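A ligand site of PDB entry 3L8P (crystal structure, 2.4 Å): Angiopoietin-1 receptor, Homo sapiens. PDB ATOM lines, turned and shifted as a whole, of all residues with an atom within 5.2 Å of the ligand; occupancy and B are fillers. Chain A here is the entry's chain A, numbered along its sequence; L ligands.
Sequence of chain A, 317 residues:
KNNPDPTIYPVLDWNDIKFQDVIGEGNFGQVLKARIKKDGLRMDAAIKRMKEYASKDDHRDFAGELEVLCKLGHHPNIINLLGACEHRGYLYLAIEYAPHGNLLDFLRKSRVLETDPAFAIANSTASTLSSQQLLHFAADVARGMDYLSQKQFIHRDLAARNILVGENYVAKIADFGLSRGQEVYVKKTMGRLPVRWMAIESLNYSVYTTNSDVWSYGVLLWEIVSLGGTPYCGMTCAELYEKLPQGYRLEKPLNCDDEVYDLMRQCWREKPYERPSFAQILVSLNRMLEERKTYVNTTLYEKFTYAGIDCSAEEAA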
ATOM      1  N   ILE A  23       3.926 -23.868 -22.566  1.00  0.00           N
ATOM      2  CA  ILE A  23       4.847 -23.690 -23.682  1.00  0.00           C
ATOM      3  C   ILE A  23       6.265 -24.181 -23.419  1.00  0.00           C
ATOM      4  O   ILE A  23       7.108 -24.179 -24.309  1.00  0.00           O
ATOM      5  CB  ILE A  23       4.884 -22.214 -24.128  1.00  0.00           C
ATOM      6  CG1 ILE A  23       5.061 -21.300 -22.908  1.00  0.00           C
ATOM      7  CG2 ILE A  23       3.581 -21.884 -24.877  1.00  0.00           C
ATOM      8  CD1 ILE A  23       5.052 -19.819 -23.243  1.00  0.00           C
ATOM      9  N   GLY A  24       6.519 -24.608 -22.190  1.00  0.00           N
ATOM     10  CA  GLY A  24       7.837 -25.082 -21.838  1.00  0.00           C
ATOM     11  C   GLY A  24       7.981 -25.326 -20.353  1.00  0.00           C
ATOM     12  O   GLY A  24       7.013 -25.214 -19.591  1.00  0.00           O
ATOM     13  N   GLU A  25       9.196 -25.649 -19.943  1.00  0.00           N
ATOM     14  CA  GLU A  25       9.476 -25.934 -18.548  1.00  0.00           C
ATOM     15  C   GLU A  25      10.936 -25.665 -18.177  1.00  0.00           C
ATOM     16  O   GLU A  25      11.851 -26.129 -18.850  1.00  0.00           O
ATOM     17  CB  GLU A  25       9.157 -27.401 -18.240  1.00  0.00           C
ATOM     18  CG  GLU A  25       9.375 -27.788 -16.801  1.00  0.00           C
ATOM     19  CD  GLU A  25       9.287 -29.277 -16.581  1.00  0.00           C
ATOM     20  OE1 GLU A  25       9.237 -29.697 -15.405  1.00  0.00           O
ATOM     21  OE2 GLU A  25       9.271 -30.033 -17.587  1.00  0.00           O
ATOM     22  N   GLY A  26      11.129 -24.899 -17.103  1.00  0.00           N
ATOM     23  CA  GLY A  26      12.480 -24.603 -16.663  1.00  0.00           C
ATOM     24  C   GLY A  26      12.852 -25.444 -15.466  1.00  0.00           C
ATOM     25  O   GLY A  26      12.093 -26.324 -15.061  1.00  0.00           O
ATOM     26  N   VAL A  31       6.233 -23.184 -17.837  1.00  0.00           N
ATOM     27  CA  VAL A  31       6.029 -21.816 -18.283  1.00  0.00           C
ATOM     28  C   VAL A  31       4.715 -21.867 -19.048  1.00  0.00           C
ATOM     29  O   VAL A  31       4.480 -22.759 -19.866  1.00  0.00           O
ATOM     30  CB  VAL A  31       7.161 -21.333 -19.212  1.00  0.00           C
ATOM     31  CG1 VAL A  31       7.284 -22.255 -20.416  1.00  0.00           C
ATOM     32  CG2 VAL A  31       6.878 -19.911 -19.696  1.00  0.00           C
ATOM     33  N   ALA A  46       4.364 -14.687 -20.609  1.00  0.00           N
ATOM     34  CA  ALA A  46       4.629 -16.046 -20.172  1.00  0.00           C
ATOM     35  C   ALA A  46       4.524 -15.988 -18.652  1.00  0.00           C
ATOM     36  O   ALA A  46       4.890 -14.982 -18.034  1.00  0.00           O
ATOM     37  CB  ALA A  46       6.031 -16.469 -20.600  1.00  0.00           C
ATOM     38  N   LYS A  48       5.439 -17.877 -14.942  1.00  0.00           N
ATOM     39  CA  LYS A  48       6.289 -18.836 -14.258  1.00  0.00           C
ATOM     40  C   LYS A  48       6.100 -18.692 -12.748  1.00  0.00           C
ATOM     41  O   LYS A  48       6.222 -17.595 -12.213  1.00  0.00           O
ATOM     42  CB  LYS A  48       7.765 -18.582 -14.623  1.00  0.00           C
ATOM     43  CG  LYS A  48       8.765 -19.493 -13.948  1.00  0.00           C
ATOM     44  CD  LYS A  48       9.991 -18.704 -13.486  1.00  0.00           C
ATOM     45  CE  LYS A  48      10.940 -19.559 -12.661  1.00  0.00           C
ATOM     46  NZ  LYS A  48      12.000 -18.757 -12.001  1.00  0.00           N
ATOM     47  N   LEU A  69      15.530  -9.104  -8.713  1.00  0.00           N
ATOM     48  CA  LEU A  69      14.877  -9.241 -10.007  1.00  0.00           C
ATOM     49  C   LEU A  69      14.064  -7.995 -10.344  1.00  0.00           C
ATOM     50  O   LEU A  69      14.220  -7.399 -11.412  1.00  0.00           O
ATOM     51  CB  LEU A  69      13.973 -10.476 -10.012  1.00  0.00           C
ATOM     52  CG  LEU A  69      13.621 -11.141 -11.341  1.00  0.00           C
ATOM     53  CD1 LEU A  69      12.664 -12.283 -11.069  1.00  0.00           C
ATOM     54  CD2 LEU A  69      12.986 -10.147 -12.299  1.00  0.00           C
ATOM     55  N   ILE A  79      15.289 -11.048 -20.905  1.00  0.00           N
ATOM     56  CA  ILE A  79      13.838 -11.191 -20.935  1.00  0.00           C
ATOM     57  C   ILE A  79      13.322 -10.315 -19.786  1.00  0.00           C
ATOM     58  O   ILE A  79      13.834 -10.362 -18.664  1.00  0.00           O
ATOM     59  CB  ILE A  79      13.402 -12.685 -20.776  1.00  0.00           C
ATOM     60  CG1 ILE A  79      11.982 -12.852 -21.304  1.00  0.00           C
ATOM     61  CG2 ILE A  79      13.515 -13.143 -19.333  1.00  0.00           C
ATOM     62  CD1 ILE A  79      11.850 -12.528 -22.778  1.00  0.00           C
ATOM     63  N   LEU A  93       5.118 -14.991 -11.659  1.00  0.00           N
ATOM     64  CA  LEU A  93       5.779 -13.934 -12.434  1.00  0.00           C
ATOM     65  C   LEU A  93       5.225 -13.852 -13.849  1.00  0.00           C
ATOM     66  O   LEU A  93       5.070 -14.880 -14.524  1.00  0.00           O
ATOM     67  CB  LEU A  93       7.288 -14.186 -12.502  1.00  0.00           C
ATOM     68  CG  LEU A  93       8.193 -13.834 -11.324  1.00  0.00           C
ATOM     69  CD1 LEU A  93       7.562 -14.238 -10.013  1.00  0.00           C
ATOM     70  CD2 LEU A  93       9.530 -14.521 -11.510  1.00  0.00           C
ATOM     71  N   ILE A  95       6.063 -12.622 -17.381  1.00  0.00           N
ATOM     72  CA  ILE A  95       7.248 -12.314 -18.168  1.00  0.00           C
ATOM     73  C   ILE A  95       6.979 -11.883 -19.605  1.00  0.00           C
ATOM     74  O   ILE A  95       6.049 -12.354 -20.249  1.00  0.00           O
ATOM     75  CB  ILE A  95       8.185 -13.535 -18.207  1.00  0.00           C
ATOM     76  CG1 ILE A  95       8.286 -14.152 -16.815  1.00  0.00           C
ATOM     77  CG2 ILE A  95       9.561 -13.144 -18.739  1.00  0.00           C
ATOM     78  CD1 ILE A  95       8.805 -13.185 -15.758  1.00  0.00           C
ATOM     79  N   GLU A  96       7.831 -10.985 -20.099  1.00  0.00           N
ATOM     80  CA  GLU A  96       7.743 -10.500 -21.464  1.00  0.00           C
ATOM     81  C   GLU A  96       7.666 -11.755 -22.326  1.00  0.00           C
ATOM     82  O   GLU A  96       8.364 -12.732 -22.050  1.00  0.00           O
ATOM     83  CB  GLU A  96       9.014  -9.714 -21.795  1.00  0.00           C
ATOM     84  CG  GLU A  96       9.196  -9.375 -23.263  1.00  0.00           C
ATOM     85  CD  GLU A  96      10.607  -8.917 -23.556  1.00  0.00           C
ATOM     86  OE1 GLU A  96      11.344  -8.623 -22.593  1.00  0.00           O
ATOM     87  OE2 GLU A  96      10.987  -8.858 -24.752  1.00  0.00           O
ATOM     88  N   TYR A  97       6.842 -11.724 -23.363  1.00  0.00           N
ATOM     89  CA  TYR A  97       6.679 -12.891 -24.211  1.00  0.00           C
ATOM     90  C   TYR A  97       7.629 -12.978 -25.407  1.00  0.00           C
ATOM     91  O   TYR A  97       7.822 -11.993 -26.132  1.00  0.00           O
ATOM     92  CB  TYR A  97       5.216 -12.949 -24.687  1.00  0.00           C
ATOM     93  CG  TYR A  97       4.882 -14.143 -25.538  1.00  0.00           C
ATOM     94  CD1 TYR A  97       5.087 -15.451 -25.063  1.00  0.00           C
ATOM     95  CD2 TYR A  97       4.383 -13.988 -26.829  1.00  0.00           C
ATOM     96  CE1 TYR A  97       4.789 -16.555 -25.864  1.00  0.00           C
ATOM     97  CE2 TYR A  97       4.083 -15.078 -27.629  1.00  0.00           C
ATOM     98  CZ  TYR A  97       4.288 -16.365 -27.144  1.00  0.00           C
ATOM     99  OH  TYR A  97       4.014 -17.437 -27.951  1.00  0.00           O
ATOM    100  N   ALA A  98       8.236 -14.143 -25.599  1.00  0.00           N
ATOM    101  CA  ALA A  98       9.148 -14.385 -26.713  1.00  0.00           C
ATOM    102  C   ALA A  98       8.432 -15.350 -27.661  1.00  0.00           C
ATOM    103  O   ALA A  98       8.508 -16.564 -27.506  1.00  0.00           O
ATOM    104  CB  ALA A  98      10.440 -15.001 -26.214  1.00  0.00           C
ATOM    105  N   PRO A  99       7.734 -14.805 -28.660  1.00  0.00           N
ATOM    106  CA  PRO A  99       6.977 -15.598 -29.632  1.00  0.00           C
ATOM    107  C   PRO A  99       7.716 -16.703 -30.361  1.00  0.00           C
ATOM    108  O   PRO A  99       7.121 -17.723 -30.704  1.00  0.00           O
ATOM    109  CB  PRO A  99       6.416 -14.530 -30.589  1.00  0.00           C
ATOM    110  CG  PRO A  99       7.414 -13.445 -30.523  1.00  0.00           C
ATOM    111  CD  PRO A  99       7.756 -13.375 -29.051  1.00  0.00           C
ATOM    112  N   HIS A 100       9.010 -16.523 -30.585  1.00  0.00           N
ATOM    113  CA  HIS A 100       9.752 -17.540 -31.320  1.00  0.00           C
ATOM    114  C   HIS A 100      10.281 -18.720 -30.501  1.00  0.00           C
ATOM    115  O   HIS A 100      10.772 -19.685 -31.076  1.00  0.00           O
ATOM    116  CB  HIS A 100      10.856 -16.852 -32.108  1.00  0.00           C
ATOM    117  CG  HIS A 100      10.355 -15.778 -33.019  1.00  0.00           C
ATOM    118  ND1 HIS A 100       9.590 -16.045 -34.128  1.00  0.00           N
ATOM    119  CD2 HIS A 100      10.418 -14.423 -32.914  1.00  0.00           C
ATOM    120  CE1 HIS A 100       9.204 -14.913 -34.681  1.00  0.00           C
ATOM    121  NE2 HIS A 100       9.696 -13.909 -33.960  1.00  0.00           N
ATOM    122  N   GLY A 101      10.187 -18.650 -29.176  1.00  0.00           N
ATOM    123  CA  GLY A 101      10.639 -19.759 -28.356  1.00  0.00           C
ATOM    124  C   GLY A 101      12.111 -19.778 -27.977  1.00  0.00           C
ATOM    125  O   GLY A 101      12.829 -18.800 -28.217  1.00  0.00           O
ATOM    126  N   ASN A 102      12.574 -20.886 -27.384  1.00  0.00           N
ATOM    127  CA  ASN A 102      13.976 -20.976 -26.969  1.00  0.00           C
ATOM    128  C   ASN A 102      14.883 -21.140 -28.172  1.00  0.00           C
ATOM    129  O   ASN A 102      14.512 -21.744 -29.180  1.00  0.00           O
ATOM    130  CB  ASN A 102      14.180 -22.132 -25.964  1.00  0.00           C
ATOM    131  CG  ASN A 102      14.163 -23.494 -26.609  1.00  0.00           C
ATOM    132  OD1 ASN A 102      15.107 -23.872 -27.307  1.00  0.00           O
ATOM    133  ND2 ASN A 102      13.096 -24.256 -26.358  1.00  0.00           N
ATOM    134  N   ARG A 161      19.165 -23.534 -24.731  1.00  0.00           N
ATOM    135  CA  ARG A 161      17.820 -23.761 -24.209  1.00  0.00           C
ATOM    136  C   ARG A 161      17.321 -22.611 -23.311  1.00  0.00           C
ATOM    137  O   ARG A 161      16.105 -22.416 -23.160  1.00  0.00           O
ATOM    138  CB  ARG A 161      17.742 -25.087 -23.430  1.00  0.00           C
ATOM    139  CG  ARG A 161      18.726 -25.192 -22.267  1.00  0.00           C
ATOM    140  CD  ARG A 161      18.587 -26.486 -21.461  1.00  0.00           C
ATOM    141  NE  ARG A 161      19.576 -26.490 -20.380  1.00  0.00           N
ATOM    142  CZ  ARG A 161      20.873 -26.752 -20.548  1.00  0.00           C
ATOM    143  NH1 ARG A 161      21.346 -27.033 -21.751  1.00  0.00           N
ATOM    144  NH2 ARG A 161      21.703 -26.658 -19.522  1.00  0.00           N
ATOM    145  N   ASN A 162      18.240 -21.850 -22.729  1.00  0.00           N
ATOM    146  CA  ASN A 162      17.839 -20.749 -21.853  1.00  0.00           C
ATOM    147  C   ASN A 162      17.867 -19.396 -22.524  1.00  0.00           C
ATOM    148  O   ASN A 162      17.790 -18.360 -21.855  1.00  0.00           O
ATOM    149  CB  ASN A 162      18.688 -20.722 -20.582  1.00  0.00           C
ATOM    150  CG  ASN A 162      18.381 -21.868 -19.661  1.00  0.00           C
ATOM    151  OD1 ASN A 162      17.229 -22.306 -19.562  1.00  0.00           O
ATOM    152  ND2 ASN A 162      19.388 -22.356 -18.964  1.00  0.00           N
ATOM    153  N   LEU A 164      16.030 -16.972 -25.290  1.00  0.00           N
ATOM    154  CA  LEU A 164      14.754 -16.815 -25.970  1.00  0.00           C
ATOM    155  C   LEU A 164      14.918 -15.974 -27.213  1.00  0.00           C
ATOM    156  O   LEU A 164      15.768 -15.090 -27.263  1.00  0.00           O
ATOM    157  CB  LEU A 164      13.744 -16.167 -25.031  1.00  0.00           C
ATOM    158  CG  LEU A 164      13.556 -16.942 -23.732  1.00  0.00           C
ATOM    159  CD1 LEU A 164      12.618 -16.181 -22.809  1.00  0.00           C
ATOM    160  CD2 LEU A 164      13.022 -18.342 -24.043  1.00  0.00           C
ATOM    161  N   ALA A 174      17.395 -15.733 -20.373  1.00  0.00           N
ATOM    162  CA  ALA A 174      16.422 -16.118 -19.351  1.00  0.00           C
ATOM    163  C   ALA A 174      17.022 -17.043 -18.309  1.00  0.00           C
ATOM    164  O   ALA A 174      18.167 -17.497 -18.430  1.00  0.00           O
ATOM    165  CB  ALA A 174      15.210 -16.788 -20.004  1.00  0.00           C
ATOM    166  N   ASP A 175      16.231 -17.322 -17.272  1.00  0.00           N
ATOM    167  CA  ASP A 175      16.609 -18.242 -16.210  1.00  0.00           C
ATOM    168  C   ASP A 175      17.990 -17.978 -15.594  1.00  0.00           C
ATOM    169  O   ASP A 175      18.709 -18.930 -15.277  1.00  0.00           O
ATOM    170  CB  ASP A 175      16.551 -19.671 -16.739  1.00  0.00           C
ATOM    171  CG  ASP A 175      16.209 -20.679 -15.673  1.00  0.00           C
ATOM    172  OD1 ASP A 175      16.342 -21.904 -15.941  1.00  0.00           O
ATOM    173  OD2 ASP A 175      15.807 -20.259 -14.559  1.00  0.00           O
ATOM    174  N   PHE A 176      18.350 -16.712 -15.434  1.00  0.00           N
ATOM    175  CA  PHE A 176      19.647 -16.384 -14.838  1.00  0.00           C
ATOM    176  C   PHE A 176      19.550 -16.405 -13.307  1.00  0.00           C
ATOM    177  O   PHE A 176      18.525 -16.024 -12.737  1.00  0.00           O
ATOM    178  CB  PHE A 176      20.138 -15.016 -15.341  1.00  0.00           C
ATOM    179  CG  PHE A 176      19.080 -13.937 -15.315  1.00  0.00           C
ATOM    180  CD1 PHE A 176      18.857 -13.207 -14.154  1.00  0.00           C
ATOM    181  CD2 PHE A 176      18.304 -13.678 -16.429  1.00  0.00           C
ATOM    182  CE1 PHE A 176      17.855 -12.224 -14.115  1.00  0.00           C
ATOM    183  CE2 PHE A 176      17.308 -12.706 -16.410  1.00  0.00           C
ATOM    184  CZ  PHE A 176      17.084 -11.976 -15.249  1.00  0.00           C
HETATM  185  C1  LIG L   1      10.706 -18.385 -20.397  1.00  0.00           C
HETATM  186  N1  LIG L   1       8.058 -21.053 -25.610  1.00  0.00           N
HETATM  187  O1  LIG L   1       8.047 -16.292 -23.827  1.00  0.00           O
HETATM  188  C2  LIG L   1      10.829 -19.730 -20.866  1.00  0.00           C
HETATM  189  N2  LIG L   1       7.838 -19.817 -26.103  1.00  0.00           N
HETATM  190  O2  LIG L   1      14.051 -15.776 -16.435  1.00  0.00           O
HETATM  191  C3  LIG L   1      10.180 -20.097 -22.118  1.00  0.00           C
HETATM  192  N3  LIG L   1       8.945 -15.490 -21.913  1.00  0.00           N
HETATM  193  C4  LIG L   1       9.427 -19.086 -22.866  1.00  0.00           C
HETATM  194  N4  LIG L   1      11.606 -20.489 -19.962  1.00  0.00           N
HETATM  195  C5  LIG L   1       8.767 -19.551 -24.193  1.00  0.00           C
HETATM  196  C6  LIG L   1       8.604 -20.974 -24.480  1.00  0.00           C
HETATM  197  C7  LIG L   1       8.254 -18.920 -25.264  1.00  0.00           C
HETATM  198  C8  LIG L   1       7.214 -19.555 -27.385  1.00  0.00           C
HETATM  199  C9  LIG L   1       9.041 -22.061 -23.545  1.00  0.00           C
HETATM  200  C10 LIG L   1      10.254 -21.550 -22.710  1.00  0.00           C
HETATM  201  C11 LIG L   1       9.347 -17.752 -22.346  1.00  0.00           C
HETATM  202  C12 LIG L   1       9.965 -17.391 -21.121  1.00  0.00           C
HETATM  203  C13 LIG L   1       9.739 -15.923 -20.780  1.00  0.00           C
HETATM  204  C14 LIG L   1       8.699 -16.459 -22.797  1.00  0.00           C
HETATM  205  C15 LIG L   1      12.736 -21.455 -20.226  1.00  0.00           C
HETATM  206  C16 LIG L   1      12.353 -22.960 -20.135  1.00  0.00           C
HETATM  207  C17 LIG L   1      13.519 -21.182 -21.545  1.00  0.00           C
HETATM  208  C18 LIG L   1      11.939 -19.585 -18.967  1.00  0.00           C
HETATM  209  C19 LIG L   1      11.411 -18.299 -19.191  1.00  0.00           C
HETATM  210  C20 LIG L   1      11.661 -17.227 -18.274  1.00  0.00           C
HETATM  211  C21 LIG L   1      12.461 -17.486 -17.100  1.00  0.00           C
HETATM  212  C22 LIG L   1      12.805 -16.423 -16.054  1.00  0.00           C
HETATM  213  C23 LIG L   1      11.743 -15.307 -15.769  1.00  0.00           C
HETATM  214  C24 LIG L   1      12.266 -14.363 -14.654  1.00  0.00           C
HETATM  215  C25 LIG L   1      13.621 -13.736 -15.097  1.00  0.00           C
HETATM  216  C26 LIG L   1      14.613 -14.887 -15.442  1.00  0.00           C
HETATM  217  C27 LIG L   1      12.976 -18.785 -16.887  1.00  0.00           C
HETATM  218  C28 LIG L   1      12.739 -19.843 -17.792  1.00  0.00           C
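N of Asp 175 lies within hydrogen-bond range of O2 of the ligand, at 2.8 Å. An oxygen (O1) of the ligand is in hydrogen-bond range of the backbone NH (N) of Ala 98 (2.8 Å).
N of Ile 23 lies within hydrogen-bond range of O of Val 31 (3.0 Å). The backbone carbonyl oxygen (O) of Asn 162 is in hydrogen-bond range of the backbone NH (N) of Ala 174. N of Val 31 sits at hydrogen-bond distance from O of Gly 24 (2.8 Å). O of Ala 46 sits at hydrogen-bond distance from N of Ile 95.
The backbone carbonyl oxygen (O) of Glu 96 lies close to a nitrogen (N3) of the ligand, at 2.8 Å. Ile 23 touches the ligand (O to C9, 3.0 Å). Gly 24 touches the ligand (CA to C9, 3.7 Å). Glu 25 touches the ligand (O to C16, 3.5 Å). Gly 26 touches the ligand (N to C16, 3.8 Å). CG1 of Val 31 touches C9 of the ligand (3.6 Å). CB of Ala 46 touches N3 of the ligand, 3.3 Å away. CG1 of Ile 79 touches C13 of the ligand, 3.8 Å away. Ile 95 touches the ligand (CG2 to C13, 3.5 Å). Tyr 97 touches the ligand. Pro 99 touches the ligand (O to C8, 3.8 Å). Gly 101 touches the ligand. O of Arg 161 touches C17 of the ligand (3.3 Å). Leu 164 touches the ligand (CD1 to C12, 3.4 Å). Ala 174 touches the ligand (C to O2, 3.7 Å). Phe 176 touches the ligand (CE2 to C26, 3.6 Å). Hydrophobic or aromatic side chains within 4 Å of the ligand: Ile 23, Val 31, Ala 46, Ile 79, Ile 95, Tyr 97, Ala 98, Leu 164, Ala 174 and Phe 176. 18 residues have an atom within 4 Å of the ligand: Ile 23, Gly 24, Glu 25, Gly 26, Val 31, Ala 46, Ile 79, Ile 95, Glu 96, Tyr 97, Ala 98, Pro 99, Gly 101, Arg 161, Leu 164, Ala 174, Asp 175 and Phe 176. The nearest printed residue that does not touch the ligand is Leu 69 (4.2 Å).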
